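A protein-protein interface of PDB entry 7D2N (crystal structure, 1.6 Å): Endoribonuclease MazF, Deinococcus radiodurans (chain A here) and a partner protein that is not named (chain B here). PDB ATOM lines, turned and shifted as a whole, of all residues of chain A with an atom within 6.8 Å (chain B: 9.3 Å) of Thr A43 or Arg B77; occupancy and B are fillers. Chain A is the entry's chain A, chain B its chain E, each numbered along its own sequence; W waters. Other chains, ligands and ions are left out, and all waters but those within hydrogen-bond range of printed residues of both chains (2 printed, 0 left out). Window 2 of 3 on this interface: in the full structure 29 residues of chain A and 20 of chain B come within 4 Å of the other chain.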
ATOM      1  N   ALA A  38     -23.938   0.884  -5.734  1.00  0.00           N
ATOM      2  CA  ALA A  38     -23.145  -0.102  -5.003  1.00  0.00           C
ATOM      3  C   ALA A  38     -21.872   0.521  -4.444  1.00  0.00           C
ATOM      4  O   ALA A  38     -21.537   0.332  -3.269  1.00  0.00           O
ATOM      5  CB  ALA A  38     -22.808  -1.290  -5.904  1.00  0.00           C
ATOM      6  N   TYR A  39     -21.160   1.294  -5.270  1.00  0.00           N
ATOM      7  CA  TYR A  39     -19.978   2.002  -4.790  1.00  0.00           C
ATOM      8  C   TYR A  39     -20.359   3.160  -3.884  1.00  0.00           C
ATOM      9  O   TYR A  39     -19.725   3.386  -2.846  1.00  0.00           O
ATOM     10  CB  TYR A  39     -19.155   2.539  -5.960  1.00  0.00           C
ATOM     11  CG  TYR A  39     -18.110   3.549  -5.510  1.00  0.00           C
ATOM     12  CD1 TYR A  39     -16.836   3.130  -5.127  1.00  0.00           C
ATOM     13  CD2 TYR A  39     -18.395   4.919  -5.475  1.00  0.00           C
ATOM     14  CE1 TYR A  39     -15.883   4.025  -4.726  1.00  0.00           C
ATOM     15  CE2 TYR A  39     -17.448   5.826  -5.064  1.00  0.00           C
ATOM     16  CZ  TYR A  39     -16.192   5.376  -4.690  1.00  0.00           C
ATOM     17  OH  TYR A  39     -15.238   6.273  -4.280  1.00  0.00           O
ATOM     18  N   ASN A  40     -21.352   3.951  -4.302  1.00  0.00           N
ATOM     19  CA  ASN A  40     -21.684   5.168  -3.567  1.00  0.00           C
ATOM     20  C   ASN A  40     -22.079   4.855  -2.133  1.00  0.00           C
ATOM     21  O   ASN A  40     -21.787   5.639  -1.218  1.00  0.00           O
ATOM     22  CB  ASN A  40     -22.810   5.921  -4.273  1.00  0.00           C
ATOM     23  CG  ASN A  40     -22.468   6.289  -5.722  1.00  0.00           C
ATOM     24  OD1 ASN A  40     -21.303   6.335  -6.117  1.00  0.00           O
ATOM     25  ND2 ASN A  40     -23.494   6.555  -6.510  1.00  0.00           N
ATOM     26  N   GLY A  41     -22.702   3.698  -1.919  1.00  0.00           N
ATOM     27  CA  GLY A  41     -23.168   3.293  -0.605  1.00  0.00           C
ATOM     28  C   GLY A  41     -22.134   2.651   0.294  1.00  0.00           C
ATOM     29  O   GLY A  41     -22.428   2.459   1.477  1.00  0.00           O
ATOM     30  N   VAL A  42     -20.950   2.297  -0.205  1.00  0.00           N
ATOM     31  CA  VAL A  42     -19.901   1.772   0.669  1.00  0.00           C
ATOM     32  C   VAL A  42     -18.750   2.738   0.857  1.00  0.00           C
ATOM     33  O   VAL A  42     -17.801   2.417   1.590  1.00  0.00           O
ATOM     34  CB  VAL A  42     -19.376   0.401   0.193  1.00  0.00           C
ATOM     35  CG1 VAL A  42     -20.484  -0.639   0.312  1.00  0.00           C
ATOM     36  CG2 VAL A  42     -18.786   0.473  -1.214  1.00  0.00           C
ATOM     37  N   THR A  43     -18.802   3.925   0.241  1.00  0.00           N
ATOM     38  CA  THR A  43     -17.786   4.941   0.454  1.00  0.00           C
ATOM     39  C   THR A  43     -18.347   6.261   0.944  1.00  0.00           C
ATOM     40  O   THR A  43     -17.598   7.049   1.532  1.00  0.00           O
ATOM     41  CB  THR A  43     -17.001   5.215  -0.839  1.00  0.00           C
ATOM     42  OG1 THR A  43     -17.901   5.711  -1.846  1.00  0.00           O
ATOM     43  CG2 THR A  43     -16.312   3.949  -1.326  1.00  0.00           C
ATOM     44  N   GLY A  44     -19.631   6.523   0.728  1.00  0.00           N
ATOM     45  CA  GLY A  44     -20.138   7.853   0.965  1.00  0.00           C
ATOM     46  C   GLY A  44     -19.695   8.870  -0.058  1.00  0.00           C
ATOM     47  O   GLY A  44     -19.964  10.064   0.110  1.00  0.00           O
ATOM     48  N   LEU A  45     -19.033   8.428  -1.118  1.00  0.00           N
ATOM     49  CA  LEU A  45     -18.559   9.286  -2.186  1.00  0.00           C
ATOM     50  C   LEU A  45     -19.258   8.903  -3.475  1.00  0.00           C
ATOM     51  O   LEU A  45     -19.874   7.844  -3.585  1.00  0.00           O
ATOM     52  CB  LEU A  45     -17.046   9.165  -2.378  1.00  0.00           C
ATOM     53  CG  LEU A  45     -16.216   9.516  -1.150  1.00  0.00           C
ATOM     54  CD1 LEU A  45     -14.845   8.887  -1.295  1.00  0.00           C
ATOM     55  CD2 LEU A  45     -16.119  11.030  -0.994  1.00  0.00           C
ATOM     56  N   MET A  46     -19.133   9.781  -4.462  1.00  0.00           N
ATOM     57  CA  MET A  46     -19.623   9.487  -5.797  1.00  0.00           C
ATOM     58  C   MET A  46     -18.796  10.284  -6.780  1.00  0.00           C
ATOM     59  O   MET A  46     -18.226  11.323  -6.439  1.00  0.00           O
ATOM     60  CB  MET A  46     -21.102   9.845  -5.956  1.00  0.00           C
ATOM     61  CG  MET A  46     -21.344  11.311  -5.752  1.00  0.00           C
ATOM     62  SD  MET A  46     -23.081  11.679  -5.909  1.00  0.00           S
ATOM     63  CE  MET A  46     -22.977  13.427  -6.084  1.00  0.00           C
ATOM     64  N   SER A  81     -14.816  13.459  -7.553  1.00  0.00           N
ATOM     65  CA  SER A  81     -15.232  12.699  -6.377  1.00  0.00           C
ATOM     66  C   SER A  81     -15.751  13.629  -5.285  1.00  0.00           C
ATOM     67  O   SER A  81     -15.011  14.498  -4.811  1.00  0.00           O
ATOM     68  CB  SER A  81     -14.045  11.896  -5.857  1.00  0.00           C
ATOM     69  OG  SER A  81     -14.348  11.276  -4.621  1.00  0.00           O
ATOM     70  N   LEU A  82     -17.003  13.430  -4.864  1.00  0.00           N
ATOM     71  CA  LEU A  82     -17.643  14.301  -3.883  1.00  0.00           C
ATOM     72  C   LEU A  82     -18.366  13.467  -2.836  1.00  0.00           C
ATOM     73  O   LEU A  82     -18.922  12.412  -3.143  1.00  0.00           O
ATOM     74  CB  LEU A  82     -18.641  15.258  -4.561  1.00  0.00           C
ATOM     75  CG  LEU A  82     -17.997  16.203  -5.578  1.00  0.00           C
ATOM     76  CD1 LEU A  82     -19.070  16.866  -6.433  1.00  0.00           C
ATOM     77  CD2 LEU A  82     -17.150  17.238  -4.864  1.00  0.00           C
ATOM     78  N   ASP A  83     -18.364  13.957  -1.591  1.00  0.00           N
ATOM     79  CA  ASP A  83     -19.062  13.283  -0.495  1.00  0.00           C
ATOM     80  C   ASP A  83     -20.531  13.684  -0.526  1.00  0.00           C
ATOM     81  O   ASP A  83     -20.888  14.807  -0.138  1.00  0.00           O
ATOM     82  CB  ASP A  83     -18.419  13.629   0.848  1.00  0.00           C
ATOM     83  CG  ASP A  83     -18.995  12.810   2.012  1.00  0.00           C
ATOM     84  OD1 ASP A  83     -20.235  12.719   2.133  1.00  0.00           O
ATOM     85  OD2 ASP A  83     -18.204  12.247   2.800  1.00  0.00           O
ATOM     86  N   TRP A  84     -21.392  12.755  -0.947  1.00  0.00           N
ATOM     87  CA  TRP A  84     -22.794  13.086  -1.146  1.00  0.00           C
ATOM     88  C   TRP A  84     -23.579  13.122   0.153  1.00  0.00           C
ATOM     89  O   TRP A  84     -24.671  13.683   0.165  1.00  0.00           O
ATOM     90  CB  TRP A  84     -23.450  12.102  -2.130  1.00  0.00           C
ATOM     91  CG  TRP A  84     -23.292  10.652  -1.753  1.00  0.00           C
ATOM     92  CD1 TRP A  84     -22.307   9.795  -2.162  1.00  0.00           C
ATOM     93  CD2 TRP A  84     -24.151   9.893  -0.887  1.00  0.00           C
ATOM     94  NE1 TRP A  84     -22.501   8.550  -1.603  1.00  0.00           N
ATOM     95  CE2 TRP A  84     -23.628   8.586  -0.820  1.00  0.00           C
ATOM     96  CE3 TRP A  84     -25.313  10.196  -0.169  1.00  0.00           C
ATOM     97  CZ2 TRP A  84     -24.218   7.582  -0.047  1.00  0.00           C
ATOM     98  CZ3 TRP A  84     -25.908   9.192   0.590  1.00  0.00           C
ATOM     99  CH2 TRP A  84     -25.357   7.901   0.642  1.00  0.00           C
ATOM    100  N   ARG A  85     -23.056  12.547   1.246  1.00  0.00           N
ATOM    101  CA  ARG A  85     -23.735  12.702   2.534  1.00  0.00           C
ATOM    102  C   ARG A  85     -23.516  14.096   3.096  1.00  0.00           C
ATOM    103  O   ARG A  85     -24.472  14.786   3.469  1.00  0.00           O
ATOM    104  CB  ARG A  85     -23.236  11.676   3.548  1.00  0.00           C
ATOM    105  CG  ARG A  85     -23.654  10.283   3.279  1.00  0.00           C
ATOM    106  CD  ARG A  85     -22.509   9.534   2.668  1.00  0.00           C
ATOM    107  NE  ARG A  85     -21.191  10.013   3.102  1.00  0.00           N
ATOM    108  CZ  ARG A  85     -20.510   9.504   4.131  1.00  0.00           C
ATOM    109  NH1 ARG A  85     -19.314   9.984   4.444  1.00  0.00           N
ATOM    110  NH2 ARG A  85     -21.028   8.517   4.850  1.00  0.00           N
ATOM    111  N   SER A  86     -22.249  14.504   3.195  1.00  0.00           N
ATOM    112  CA  SER A  86     -21.928  15.825   3.717  1.00  0.00           C
ATOM    113  C   SER A  86     -22.589  16.917   2.890  1.00  0.00           C
ATOM    114  O   SER A  86     -23.020  17.939   3.431  1.00  0.00           O
ATOM    115  CB  SER A  86     -20.415  16.026   3.739  1.00  0.00           C
ATOM    116  OG  SER A  86     -19.825  15.258   4.768  1.00  0.00           O
ATOM    117  N   LEU B  74     -13.501  21.468   1.261  1.00  0.00           N
ATOM    118  CA  LEU B  74     -13.475  20.008   1.344  1.00  0.00           C
ATOM    119  C   LEU B  74     -14.532  19.514   2.324  1.00  0.00           C
ATOM    120  O   LEU B  74     -14.685  20.062   3.422  1.00  0.00           O
ATOM    121  CB  LEU B  74     -12.085  19.539   1.786  1.00  0.00           C
ATOM    122  CG  LEU B  74     -11.769  18.043   1.796  1.00  0.00           C
ATOM    123  CD1 LEU B  74     -10.304  17.843   1.438  1.00  0.00           C
ATOM    124  CD2 LEU B  74     -12.074  17.415   3.140  1.00  0.00           C
ATOM    125  N   GLU B  75     -15.269  18.468   1.931  1.00  0.00           N
ATOM    126  CA  GLU B  75     -16.356  17.924   2.736  1.00  0.00           C
ATOM    127  C   GLU B  75     -16.157  16.441   3.014  1.00  0.00           C
ATOM    128  O   GLU B  75     -15.743  15.687   2.130  1.00  0.00           O
ATOM    129  CB  GLU B  75     -17.717  18.105   2.043  1.00  0.00           C
ATOM    130  CG  GLU B  75     -18.092  19.538   1.795  1.00  0.00           C
ATOM    131  CD  GLU B  75     -18.599  20.225   3.048  1.00  0.00           C
ATOM    132  OE1 GLU B  75     -18.588  19.589   4.123  1.00  0.00           O
ATOM    133  OE2 GLU B  75     -19.013  21.401   2.957  1.00  0.00           O
ATOM    134  N   GLY B  76     -16.471  16.029   4.240  1.00  0.00           N
ATOM    135  CA  GLY B  76     -16.638  14.607   4.524  1.00  0.00           C
ATOM    136  C   GLY B  76     -15.405  13.788   4.218  1.00  0.00           C
ATOM    137  O   GLY B  76     -14.292  14.103   4.657  1.00  0.00           O
ATOM    138  N   ARG B  77     -15.600  12.712   3.454  1.00  0.00           N
ATOM    139  CA  ARG B  77     -14.540  11.763   3.141  1.00  0.00           C
ATOM    140  C   ARG B  77     -13.729  12.155   1.908  1.00  0.00           C
ATOM    141  O   ARG B  77     -12.912  11.351   1.440  1.00  0.00           O
ATOM    142  CB  ARG B  77     -15.139  10.363   2.965  1.00  0.00           C
ATOM    143  CG  ARG B  77     -15.986   9.928   4.158  1.00  0.00           C
ATOM    144  CD  ARG B  77     -16.314   8.449   4.109  1.00  0.00           C
ATOM    145  NE  ARG B  77     -15.146   7.624   4.397  1.00  0.00           N
ATOM    146  CZ  ARG B  77     -14.474   6.922   3.489  1.00  0.00           C
ATOM    147  NH1 ARG B  77     -14.854   6.930   2.217  1.00  0.00           N
ATOM    148  NH2 ARG B  77     -13.414   6.208   3.855  1.00  0.00           N
ATOM    149  N   GLU B  78     -13.898  13.377   1.398  1.00  0.00           N
ATOM    150  CA  GLU B  78     -13.116  13.809   0.245  1.00  0.00           C
ATOM    151  C   GLU B  78     -11.635  13.877   0.595  1.00  0.00           C
ATOM    152  O   GLU B  78     -11.255  14.404   1.643  1.00  0.00           O
ATOM    153  CB  GLU B  78     -13.612  15.170  -0.250  1.00  0.00           C
ATOM    154  CG  GLU B  78     -14.989  15.076  -0.911  1.00  0.00           C
ATOM    155  CD  GLU B  78     -15.778  16.396  -0.953  1.00  0.00           C
ATOM    156  OE1 GLU B  78     -16.994  16.316  -1.212  1.00  0.00           O
ATOM    157  OE2 GLU B  78     -15.198  17.496  -0.771  1.00  0.00           O
ATOM    158  N   GLU B  79     -10.798  13.327  -0.287  1.00  0.00           N
ATOM    159  CA  GLU B  79      -9.352  13.377  -0.094  1.00  0.00           C
ATOM    160  C   GLU B  79      -8.784  14.746  -0.447  1.00  0.00           C
ATOM    161  O   GLU B  79      -7.753  15.154   0.106  1.00  0.00           O
ATOM    162  CB  GLU B  79      -8.693  12.287  -0.942  1.00  0.00           C
ATOM    163  CG  GLU B  79      -7.183  12.200  -0.819  1.00  0.00           C
ATOM    164  CD  GLU B  79      -6.743  11.521   0.473  1.00  0.00           C
ATOM    165  OE1 GLU B  79      -7.594  10.882   1.137  1.00  0.00           O
ATOM    166  OE2 GLU B  79      -5.546  11.628   0.817  1.00  0.00           O
ATOM    167  N   TRP B  80      -9.444  15.459  -1.355  1.00  0.00           N
ATOM    168  CA  TRP B  80      -8.997  16.758  -1.838  1.00  0.00           C
ATOM    169  C   TRP B  80     -10.117  17.408  -2.650  1.00  0.00           C
ATOM    170  O   TRP B  80     -11.227  16.863  -2.689  1.00  0.00           O
ATOM    171  CB  TRP B  80      -7.734  16.612  -2.683  1.00  0.00           C
ATOM    172  CG  TRP B  80      -7.873  15.767  -3.928  1.00  0.00           C
ATOM    173  CD1 TRP B  80      -8.915  14.934  -4.278  1.00  0.00           C
ATOM    174  CD2 TRP B  80      -6.913  15.672  -4.980  1.00  0.00           C
ATOM    175  NE1 TRP B  80      -8.648  14.336  -5.495  1.00  0.00           N
ATOM    176  CE2 TRP B  80      -7.428  14.777  -5.945  1.00  0.00           C
ATOM    177  CE3 TRP B  80      -5.664  16.265  -5.205  1.00  0.00           C
ATOM    178  CZ2 TRP B  80      -6.733  14.457  -7.106  1.00  0.00           C
ATOM    179  CZ3 TRP B  80      -4.978  15.947  -6.356  1.00  0.00           C
ATOM    180  CH2 TRP B  80      -5.517  15.057  -7.299  1.00  0.00           C
HETATM  181  O   HOH W   1     -12.204  13.301  -3.193  1.00  0.00           O
HETATM  182  O   HOH W   2     -13.021  16.555  -4.693  1.00  0.00           O
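Arg B77 touches Leu A45. Glu B78 touches Ser A81. Leu A82 touches Glu B78 (CA to OE1, 3.4 Å). Glu B75 touches Asp A83. CA of Gly B76 touches OD2 of Asp A83, 3.3 Å away. Arg A85 touches Arg B77. Ser A86 touches Glu B75 (CB to CB, 3.8 Å).
The backbone carbonyl oxygen of Thr A43 sits at hydrogen-bond distance from the guanidinium group of Arg B77, at 2.8 Å. The side-chain carboxylate (OD2) of Asp A83 lies within hydrogen-bond range of the backbone NH (N) of Arg B77 (2.7 Å). The backbone NH (N) of Asp A83 lies within hydrogen-bond range of the side-chain carboxylate (OE1) of Glu B78 (2.8 Å). N of Gly B76 lies close to OG of Ser A86 (3.5 Å).
Thr A43 touches one residue of chain B. Of chain A, only Thr A43 (2.8 Å), Leu A45 (3.9 Å), Asp A83 (2.7 Å) and Arg A85 (3.3 Å) come within 4 Å of Arg B77. No residue of chain B comes within 4 Å of Gly A44. Leu A45 touches just one residue of chain B: Arg B77 (3.9 Å). Of the printed residues of chain B, Leu A82 touches Glu B78 (3.4 Å). Of the printed residues of chain A, Gly B76 touches Asp A83 and Ser A86. Met A46 touches none of the printed residues of chain B. Leu B74 touches none of the printed residues of chain A. The nearest residue of chain B that does not touch Thr A43 is Glu B78 (7.3 Å). The nearest residue of chain A that does not touch Arg B77 is Gly A44 (5.0 Å).
The backbone carbonyl oxygen of Tyr A39 lies within hydrogen-bond range of the side-chain hydroxyl of Thr A43, 3.1 Å away. The side-chain amide oxygen (OD1) of Asn A40 sits close to the backbone carbonyl oxygen (O) of Leu A45, 3.3 Å away. The guanidinium group of Arg A85 lies close to the backbone carbonyl oxygen of Gly A44 (3.2 Å). The backbone carbonyl oxygen of Leu A45 sits at hydrogen-bond distance from the indole nitrogen of Trp A84. OD2 of Asp A83 lies within salt-bridge range of NH1 of Arg A85 (3.0 Å). The side-chain carboxylate of Asp A83 lies within hydrogen-bond range of the backbone NH of Ser A86, 2.9 Å away.
Water W2 bridges the backbone carbonyl oxygen of Trp B80 (2.7 Å) and the backbone carbonyl oxygen of Ser A81 (2.9 Å). Water W1 lies within hydrogen-bond range of the backbone NH of Glu B79 (3.2 Å) and the side-chain hydroxyl of Ser A81 (3.3 Å).
Of the 7 printed residues of chain B, 4 touch a printed residue of chain A. Printed residues of chain B that touch a printed residue of chain A: Glu B75, Gly B76, Arg B77 and Glu B78. Along chain B the printed residues that touch a printed residue of chain A span positions 75 to 78. Of the 15 printed residues of chain A, 7 touch a printed residue of chain B. Among the printed residues, 11 pairs touch across the chains.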
